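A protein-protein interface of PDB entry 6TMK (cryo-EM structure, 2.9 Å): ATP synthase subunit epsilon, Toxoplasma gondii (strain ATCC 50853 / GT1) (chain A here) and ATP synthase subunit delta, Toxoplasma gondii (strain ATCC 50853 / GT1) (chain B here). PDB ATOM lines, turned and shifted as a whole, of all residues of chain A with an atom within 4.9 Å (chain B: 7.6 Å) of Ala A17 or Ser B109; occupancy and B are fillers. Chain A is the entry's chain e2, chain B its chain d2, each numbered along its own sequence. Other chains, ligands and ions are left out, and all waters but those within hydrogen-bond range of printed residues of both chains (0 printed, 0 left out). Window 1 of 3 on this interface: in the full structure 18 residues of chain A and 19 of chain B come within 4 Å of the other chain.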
ATOM      1  N   TYR A  12     -16.447  34.105  -2.317  1.00  0.00           N
ATOM      2  CA  TYR A  12     -16.023  33.837  -3.688  1.00  0.00           C
ATOM      3  C   TYR A  12     -15.131  32.603  -3.762  1.00  0.00           C
ATOM      4  O   TYR A  12     -15.323  31.736  -4.625  1.00  0.00           O
ATOM      5  CB  TYR A  12     -15.314  35.065  -4.260  1.00  0.00           C
ATOM      6  CG  TYR A  12     -14.250  34.758  -5.285  1.00  0.00           C
ATOM      7  CD1 TYR A  12     -14.587  34.463  -6.596  1.00  0.00           C
ATOM      8  CD2 TYR A  12     -12.906  34.809  -4.952  1.00  0.00           C
ATOM      9  CE1 TYR A  12     -13.618  34.193  -7.536  1.00  0.00           C
ATOM     10  CE2 TYR A  12     -11.930  34.545  -5.887  1.00  0.00           C
ATOM     11  CZ  TYR A  12     -12.290  34.237  -7.177  1.00  0.00           C
ATOM     12  OH  TYR A  12     -11.319  33.975  -8.113  1.00  0.00           O
ATOM     13  N   ALA A  13     -14.172  32.486  -2.843  1.00  0.00           N
ATOM     14  CA  ALA A  13     -13.249  31.361  -2.872  1.00  0.00           C
ATOM     15  C   ALA A  13     -13.980  30.049  -2.635  1.00  0.00           C
ATOM     16  O   ALA A  13     -13.719  29.055  -3.319  1.00  0.00           O
ATOM     17  CB  ALA A  13     -12.157  31.563  -1.827  1.00  0.00           C
ATOM     18  N   SER A  14     -14.908  30.027  -1.680  1.00  0.00           N
ATOM     19  CA  SER A  14     -15.657  28.808  -1.406  1.00  0.00           C
ATOM     20  C   SER A  14     -16.531  28.432  -2.595  1.00  0.00           C
ATOM     21  O   SER A  14     -16.551  27.273  -3.027  1.00  0.00           O
ATOM     22  CB  SER A  14     -16.505  28.990  -0.151  1.00  0.00           C
ATOM     23  OG  SER A  14     -15.713  29.446   0.931  1.00  0.00           O
ATOM     24  N   GLU A  15     -17.289  29.398  -3.121  1.00  0.00           N
ATOM     25  CA  GLU A  15     -18.198  29.118  -4.221  1.00  0.00           C
ATOM     26  C   GLU A  15     -17.459  28.742  -5.500  1.00  0.00           C
ATOM     27  O   GLU A  15     -18.058  28.116  -6.381  1.00  0.00           O
ATOM     28  CB  GLU A  15     -19.098  30.328  -4.459  1.00  0.00           C
ATOM     29  CG  GLU A  15     -20.090  30.556  -3.326  1.00  0.00           C
ATOM     30  CD  GLU A  15     -21.172  31.557  -3.673  1.00  0.00           C
ATOM     31  OE1 GLU A  15     -21.531  31.661  -4.863  1.00  0.00           O
ATOM     32  OE2 GLU A  15     -21.664  32.242  -2.752  1.00  0.00           O
ATOM     33  N   MET A  16     -16.181  29.105  -5.628  1.00  0.00           N
ATOM     34  CA  MET A  16     -15.399  28.676  -6.782  1.00  0.00           C
ATOM     35  C   MET A  16     -14.725  27.331  -6.549  1.00  0.00           C
ATOM     36  O   MET A  16     -14.607  26.524  -7.482  1.00  0.00           O
ATOM     37  CB  MET A  16     -14.335  29.725  -7.115  1.00  0.00           C
ATOM     38  CG  MET A  16     -14.881  30.998  -7.744  1.00  0.00           C
ATOM     39  SD  MET A  16     -15.753  30.754  -9.302  1.00  0.00           S
ATOM     40  CE  MET A  16     -14.483  29.967 -10.284  1.00  0.00           C
ATOM     41  N   ALA A  17     -14.300  27.067  -5.313  1.00  0.00           N
ATOM     42  CA  ALA A  17     -13.782  25.751  -4.971  1.00  0.00           C
ATOM     43  C   ALA A  17     -14.859  24.690  -5.118  1.00  0.00           C
ATOM     44  O   ALA A  17     -14.555  23.538  -5.439  1.00  0.00           O
ATOM     45  CB  ALA A  17     -13.231  25.755  -3.547  1.00  0.00           C
ATOM     46  N   ALA A  18     -16.120  25.058  -4.895  1.00  0.00           N
ATOM     47  CA  ALA A  18     -17.215  24.128  -5.142  1.00  0.00           C
ATOM     48  C   ALA A  18     -17.259  23.704  -6.606  1.00  0.00           C
ATOM     49  O   ALA A  18     -17.358  22.513  -6.918  1.00  0.00           O
ATOM     50  CB  ALA A  18     -18.540  24.762  -4.729  1.00  0.00           C
ATOM     51  N   LEU A  19     -17.223  24.672  -7.523  1.00  0.00           N
ATOM     52  CA  LEU A  19     -17.212  24.339  -8.944  1.00  0.00           C
ATOM     53  C   LEU A  19     -15.989  23.507  -9.308  1.00  0.00           C
ATOM     54  O   LEU A  19     -16.087  22.530 -10.066  1.00  0.00           O
ATOM     55  CB  LEU A  19     -17.255  25.616  -9.781  1.00  0.00           C
ATOM     56  CG  LEU A  19     -18.562  26.408  -9.736  1.00  0.00           C
ATOM     57  CD1 LEU A  19     -18.387  27.749 -10.421  1.00  0.00           C
ATOM     58  CD2 LEU A  19     -19.698  25.629 -10.377  1.00  0.00           C
ATOM     59  N   LEU A  20     -14.827  23.859  -8.758  1.00  0.00           N
ATOM     60  CA  LEU A  20     -13.643  23.048  -9.017  1.00  0.00           C
ATOM     61  C   LEU A  20     -13.852  21.615  -8.545  1.00  0.00           C
ATOM     62  O   LEU A  20     -13.492  20.663  -9.248  1.00  0.00           O
ATOM     63  CB  LEU A  20     -12.425  23.664  -8.331  1.00  0.00           C
ATOM     64  CG  LEU A  20     -11.149  22.822  -8.352  1.00  0.00           C
ATOM     65  CD1 LEU A  20     -10.803  22.406  -9.768  1.00  0.00           C
ATOM     66  CD2 LEU A  20      -9.997  23.582  -7.729  1.00  0.00           C
ATOM     67  N   ARG A  21     -14.435  21.441  -7.360  1.00  0.00           N
ATOM     68  CA  ARG A  21     -14.714  20.101  -6.863  1.00  0.00           C
ATOM     69  C   ARG A  21     -15.715  19.379  -7.752  1.00  0.00           C
ATOM     70  O   ARG A  21     -15.666  18.151  -7.879  1.00  0.00           O
ATOM     71  CB  ARG A  21     -15.240  20.189  -5.434  1.00  0.00           C
ATOM     72  CG  ARG A  21     -14.159  20.410  -4.397  1.00  0.00           C
ATOM     73  CD  ARG A  21     -14.609  19.947  -3.031  1.00  0.00           C
ATOM     74  NE  ARG A  21     -15.829  20.631  -2.614  1.00  0.00           N
ATOM     75  CZ  ARG A  21     -15.857  21.837  -2.060  1.00  0.00           C
ATOM     76  NH1 ARG A  21     -14.731  22.509  -1.861  1.00  0.00           N
ATOM     77  NH2 ARG A  21     -17.014  22.380  -1.713  1.00  0.00           N
ATOM     78  N   PRO B  68       0.184  31.171 -10.568  1.00  0.00           N
ATOM     79  CA  PRO B  68      -0.665  32.080 -11.355  1.00  0.00           C
ATOM     80  C   PRO B  68      -1.248  33.241 -10.549  1.00  0.00           C
ATOM     81  O   PRO B  68      -2.393  33.237 -10.094  1.00  0.00           O
ATOM     82  CB  PRO B  68      -1.754  31.139 -11.865  1.00  0.00           C
ATOM     83  CG  PRO B  68      -1.979  30.234 -10.695  1.00  0.00           C
ATOM     84  CD  PRO B  68      -0.608  30.046 -10.040  1.00  0.00           C
ATOM     85  N   LEU B  87      -3.894  34.932  -5.840  1.00  0.00           N
ATOM     86  CA  LEU B  87      -3.996  34.078  -7.011  1.00  0.00           C
ATOM     87  C   LEU B  87      -5.442  33.966  -7.470  1.00  0.00           C
ATOM     88  O   LEU B  87      -6.384  34.147  -6.694  1.00  0.00           O
ATOM     89  CB  LEU B  87      -3.446  32.681  -6.711  1.00  0.00           C
ATOM     90  CG  LEU B  87      -2.165  32.616  -5.880  1.00  0.00           C
ATOM     91  CD1 LEU B  87      -1.744  31.174  -5.680  1.00  0.00           C
ATOM     92  CD2 LEU B  87      -1.050  33.413  -6.519  1.00  0.00           C
ATOM     93  N   LYS B  88      -5.603  33.660  -8.755  1.00  0.00           N
ATOM     94  CA  LYS B  88      -6.900  33.671  -9.416  1.00  0.00           C
ATOM     95  C   LYS B  88      -7.328  32.285  -9.875  1.00  0.00           C
ATOM     96  O   LYS B  88      -8.457  31.865  -9.610  1.00  0.00           O
ATOM     97  CB  LYS B  88      -6.886  34.633 -10.615  1.00  0.00           C
ATOM     98  CG  LYS B  88      -5.871  34.301 -11.699  1.00  0.00           C
ATOM     99  CD  LYS B  88      -5.763  35.425 -12.719  1.00  0.00           C
ATOM    100  CE  LYS B  88      -4.770  35.092 -13.821  1.00  0.00           C
ATOM    101  NZ  LYS B  88      -4.588  36.223 -14.774  1.00  0.00           N
ATOM    102  N   ALA B  89      -6.442  31.563 -10.558  1.00  0.00           N
ATOM    103  CA  ALA B  89      -6.668  30.186 -10.976  1.00  0.00           C
ATOM    104  C   ALA B  89      -5.448  29.737 -11.766  1.00  0.00           C
ATOM    105  O   ALA B  89      -4.667  30.561 -12.250  1.00  0.00           O
ATOM    106  CB  ALA B  89      -7.932  30.035 -11.824  1.00  0.00           C
ATOM    107  N   GLY B  90      -5.299  28.421 -11.898  1.00  0.00           N
ATOM    108  CA  GLY B  90      -4.433  27.842 -12.897  1.00  0.00           C
ATOM    109  C   GLY B  90      -3.478  26.848 -12.278  1.00  0.00           C
ATOM    110  O   GLY B  90      -3.690  26.361 -11.163  1.00  0.00           O
ATOM    111  N   ILE B  92      -0.142  25.679 -10.866  1.00  0.00           N
ATOM    112  CA  ILE B  92       1.161  25.746 -10.219  1.00  0.00           C
ATOM    113  C   ILE B  92       2.063  24.660 -10.784  1.00  0.00           C
ATOM    114  O   ILE B  92       1.625  23.535 -11.057  1.00  0.00           O
ATOM    115  CB  ILE B  92       1.014  25.605  -8.696  1.00  0.00           C
ATOM    116  CG1 ILE B  92       0.179  26.750  -8.132  1.00  0.00           C
ATOM    117  CG2 ILE B  92       2.377  25.590  -8.037  1.00  0.00           C
ATOM    118  CD1 ILE B  92      -0.632  26.360  -6.933  1.00  0.00           C
ATOM    119  N   PHE B 106      -0.050  21.296 -10.375  1.00  0.00           N
ATOM    120  CA  PHE B 106      -1.151  21.333  -9.424  1.00  0.00           C
ATOM    121  C   PHE B 106      -2.054  22.496  -9.794  1.00  0.00           C
ATOM    122  O   PHE B 106      -1.574  23.615  -9.994  1.00  0.00           O
ATOM    123  CB  PHE B 106      -0.641  21.486  -7.989  1.00  0.00           C
ATOM    124  CG  PHE B 106       0.154  20.312  -7.501  1.00  0.00           C
ATOM    125  CD1 PHE B 106       1.532  20.388  -7.407  1.00  0.00           C
ATOM    126  CD2 PHE B 106      -0.473  19.132  -7.142  1.00  0.00           C
ATOM    127  CE1 PHE B 106       2.270  19.312  -6.960  1.00  0.00           C
ATOM    128  CE2 PHE B 106       0.261  18.051  -6.696  1.00  0.00           C
ATOM    129  CZ  PHE B 106       1.634  18.142  -6.607  1.00  0.00           C
ATOM    130  N   PHE B 107      -3.354  22.233  -9.881  1.00  0.00           N
ATOM    131  CA  PHE B 107      -4.332  23.277 -10.148  1.00  0.00           C
ATOM    132  C   PHE B 107      -4.829  23.894  -8.849  1.00  0.00           C
ATOM    133  O   PHE B 107      -5.189  23.177  -7.908  1.00  0.00           O
ATOM    134  CB  PHE B 107      -5.511  22.725 -10.944  1.00  0.00           C
ATOM    135  CG  PHE B 107      -6.229  23.765 -11.748  1.00  0.00           C
ATOM    136  CD1 PHE B 107      -5.787  24.110 -13.011  1.00  0.00           C
ATOM    137  CD2 PHE B 107      -7.341  24.405 -11.237  1.00  0.00           C
ATOM    138  CE1 PHE B 107      -6.445  25.067 -13.751  1.00  0.00           C
ATOM    139  CE2 PHE B 107      -8.002  25.365 -11.971  1.00  0.00           C
ATOM    140  CZ  PHE B 107      -7.554  25.695 -13.230  1.00  0.00           C
ATOM    141  N   LEU B 108      -4.846  25.222  -8.806  1.00  0.00           N
ATOM    142  CA  LEU B 108      -5.292  25.977  -7.647  1.00  0.00           C
ATOM    143  C   LEU B 108      -6.496  26.824  -8.031  1.00  0.00           C
ATOM    144  O   LEU B 108      -6.525  27.427  -9.109  1.00  0.00           O
ATOM    145  CB  LEU B 108      -4.178  26.874  -7.110  1.00  0.00           C
ATOM    146  CG  LEU B 108      -4.510  27.638  -5.831  1.00  0.00           C
ATOM    147  CD1 LEU B 108      -3.358  27.584  -4.846  1.00  0.00           C
ATOM    148  CD2 LEU B 108      -4.855  29.075  -6.165  1.00  0.00           C
ATOM    149  N   SER B 109      -7.488  26.869  -7.143  1.00  0.00           N
ATOM    150  CA  SER B 109      -8.662  27.703  -7.377  1.00  0.00           C
ATOM    151  C   SER B 109      -8.395  29.143  -6.959  1.00  0.00           C
ATOM    152  O   SER B 109      -8.398  30.056  -7.791  1.00  0.00           O
ATOM    153  CB  SER B 109      -9.864  27.140  -6.620  1.00  0.00           C
ATOM    154  OG  SER B 109     -10.898  28.103  -6.522  1.00  0.00           O
ATOM    155  N   ASP B 110      -8.148  29.357  -5.669  1.00  0.00           N
ATOM    156  CA  ASP B 110      -7.994  30.692  -5.115  1.00  0.00           C
ATOM    157  C   ASP B 110      -7.143  30.590  -3.860  1.00  0.00           C
ATOM    158  O   ASP B 110      -7.061  29.534  -3.228  1.00  0.00           O
ATOM    159  CB  ASP B 110      -9.351  31.328  -4.794  1.00  0.00           C
ATOM    160  CG  ASP B 110     -10.100  31.761  -6.037  1.00  0.00           C
ATOM    161  OD1 ASP B 110      -9.450  32.230  -6.994  1.00  0.00           O
ATOM    162  OD2 ASP B 110     -11.340  31.621  -6.062  1.00  0.00           O
ATOM    163  N   GLY B 111      -6.516  31.692  -3.505  1.00  0.00           N
ATOM    164  CA  GLY B 111      -5.734  31.740  -2.289  1.00  0.00           C
ATOM    165  C   GLY B 111      -4.637  32.782  -2.402  1.00  0.00           C
ATOM    166  O   GLY B 111      -4.774  33.766  -3.126  1.00  0.00           O
ATOM    167  N   LEU B 130      -0.814  28.848  -0.397  1.00  0.00           N
ATOM    168  CA  LEU B 130      -2.043  28.427   0.259  1.00  0.00           C
ATOM    169  C   LEU B 130      -3.188  28.450  -0.742  1.00  0.00           C
ATOM    170  O   LEU B 130      -3.416  29.462  -1.412  1.00  0.00           O
ATOM    171  CB  LEU B 130      -2.367  29.334   1.445  1.00  0.00           C
ATOM    172  CG  LEU B 130      -1.177  29.762   2.301  1.00  0.00           C
ATOM    173  CD1 LEU B 130      -1.616  30.757   3.359  1.00  0.00           C
ATOM    174  CD2 LEU B 130      -0.523  28.550   2.934  1.00  0.00           C
ATOM    175  N   GLY B 131      -3.893  27.339  -0.838  1.00  0.00           N
ATOM    176  CA  GLY B 131      -4.996  27.211  -1.776  1.00  0.00           C
ATOM    177  C   GLY B 131      -6.218  26.621  -1.110  1.00  0.00           C
ATOM    178  O   GLY B 131      -6.119  25.671  -0.337  1.00  0.00           O
ATOM    179  N   VAL B 132      -7.379  27.201  -1.418  1.00  0.00           N
ATOM    180  CA  VAL B 132      -8.622  26.721  -0.831  1.00  0.00           C
ATOM    181  C   VAL B 132      -8.989  25.348  -1.376  1.00  0.00           C
ATOM    182  O   VAL B 132      -9.709  24.592  -0.714  1.00  0.00           O
ATOM    183  CB  VAL B 132      -9.756  27.730  -1.082  1.00  0.00           C
ATOM    184  CG1 VAL B 132     -11.016  27.312  -0.348  1.00  0.00           C
ATOM    185  CG2 VAL B 132      -9.325  29.116  -0.641  1.00  0.00           C
ATOM    186  N   GLU B 133      -8.510  25.008  -2.570  1.00  0.00           N
ATOM    187  CA  GLU B 133      -8.704  23.670  -3.123  1.00  0.00           C
ATOM    188  C   GLU B 133      -7.585  23.436  -4.127  1.00  0.00           C
ATOM    189  O   GLU B 133      -7.600  24.021  -5.215  1.00  0.00           O
ATOM    190  CB  GLU B 133     -10.072  23.538  -3.777  1.00  0.00           C
ATOM    191  CG  GLU B 133     -10.487  22.103  -4.042  1.00  0.00           C
ATOM    192  CD  GLU B 133     -10.941  21.384  -2.788  1.00  0.00           C
ATOM    193  OE1 GLU B 133     -12.021  21.725  -2.263  1.00  0.00           O
ATOM    194  OE2 GLU B 133     -10.217  20.475  -2.327  1.00  0.00           O
ATOM    195  N   VAL B 134      -6.628  22.591  -3.763  1.00  0.00           N
ATOM    196  CA  VAL B 134      -5.460  22.310  -4.590  1.00  0.00           C
ATOM    197  C   VAL B 134      -5.539  20.861  -5.045  1.00  0.00           C
ATOM    198  O   VAL B 134      -5.358  19.937  -4.242  1.00  0.00           O
ATOM    199  CB  VAL B 134      -4.155  22.579  -3.831  1.00  0.00           C
ATOM    200  CG1 VAL B 134      -2.979  21.965  -4.568  1.00  0.00           C
ATOM    201  CG2 VAL B 134      -3.955  24.066  -3.643  1.00  0.00           C
ATOM    202  N   VAL B 135      -5.807  20.660  -6.330  1.00  0.00           N
ATOM    203  CA  VAL B 135      -5.850  19.321  -6.911  1.00  0.00           C
ATOM    204  C   VAL B 135      -4.607  19.155  -7.776  1.00  0.00           C
ATOM    205  O   VAL B 135      -4.017  20.157  -8.202  1.00  0.00           O
ATOM    206  CB  VAL B 135      -7.134  19.105  -7.727  1.00  0.00           C
ATOM    207  CG1 VAL B 135      -7.308  17.636  -8.071  1.00  0.00           C
ATOM    208  CG2 VAL B 135      -8.336  19.620  -6.965  1.00  0.00           C
ATOM    209  N   LEU B 174     -12.544  30.203 -14.528  1.00  0.00           N
ATOM    210  CA  LEU B 174     -11.888  29.063 -13.903  1.00  0.00           C
ATOM    211  C   LEU B 174     -12.074  27.799 -14.730  1.00  0.00           C
ATOM    212  O   LEU B 174     -11.156  26.981 -14.831  1.00  0.00           O
ATOM    213  CB  LEU B 174     -12.413  28.865 -12.483  1.00  0.00           C
ATOM    214  CG  LEU B 174     -11.591  27.892 -11.634  1.00  0.00           C
ATOM    215  CD1 LEU B 174     -11.591  28.311 -10.174  1.00  0.00           C
ATOM    216  CD2 LEU B 174     -12.116  26.474 -11.769  1.00  0.00           C
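The side-chain hydroxyl of Tyr A12 is in hydrogen-bond range of the side-chain carboxylate of Asp B110 (2.8 Å).
The side-chain carboxylate (OE1) of Glu B133 lies within salt-bridge range of the guanidinium group (NH1) of Arg A21 (2.8 Å).
The backbone carbonyl oxygen of Ser B109 sits close to the backbone carbonyl oxygen of Lys B88, 2.6 Å away.
The backbone NH (N) of Ser B109 sits at hydrogen-bond distance from the backbone carbonyl oxygen (O) of Glu B133 (3.4 Å).
N of Val B132 sits at hydrogen-bond distance from O of Asp B110.
Among the printed residues, pairs that only touch across the chains: Met A16 with Leu B174, Leu A20 with Glu B133, Met A16 with Asp B110, Ala A13 with Asp B110, Leu A20 with Ser B109, Ala A17 with Ser B109, Met A16 with Ser B109, Tyr A12 with Lys B88, Ala A17 with Glu B133 and Ala A13 with Val B132.
Ala A17 touches two residues of chain B.
Ser B109 touches just these residues of chain A: Met A16 (3.8 Å), Ala A17 (3.8 Å) and Leu A20 (3.7 Å).
Printed residues of chain B within 4 Å of Met A16: Ser B109, Asp B110 and Leu B174.
Printed residues of chain B within 4 Å of Ala A13: Asp B110 and Val B132.
Of the printed residues of chain B, Leu A20 touches Ser B109 (3.7 Å) and Glu B133 (3.5 Å).
Gly B111 touches none of the printed residues of chain A.
Ile B92 touches none of the printed residues of chain A.
Among the printed residues, 12 pairs touch across the chains.
Among the printed residues, Asp or Glu carboxylates within 4 Å of a Lys or Arg side-chain nitrogen of the other chain: Arg A21 with Glu B133 (2.8 Å).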
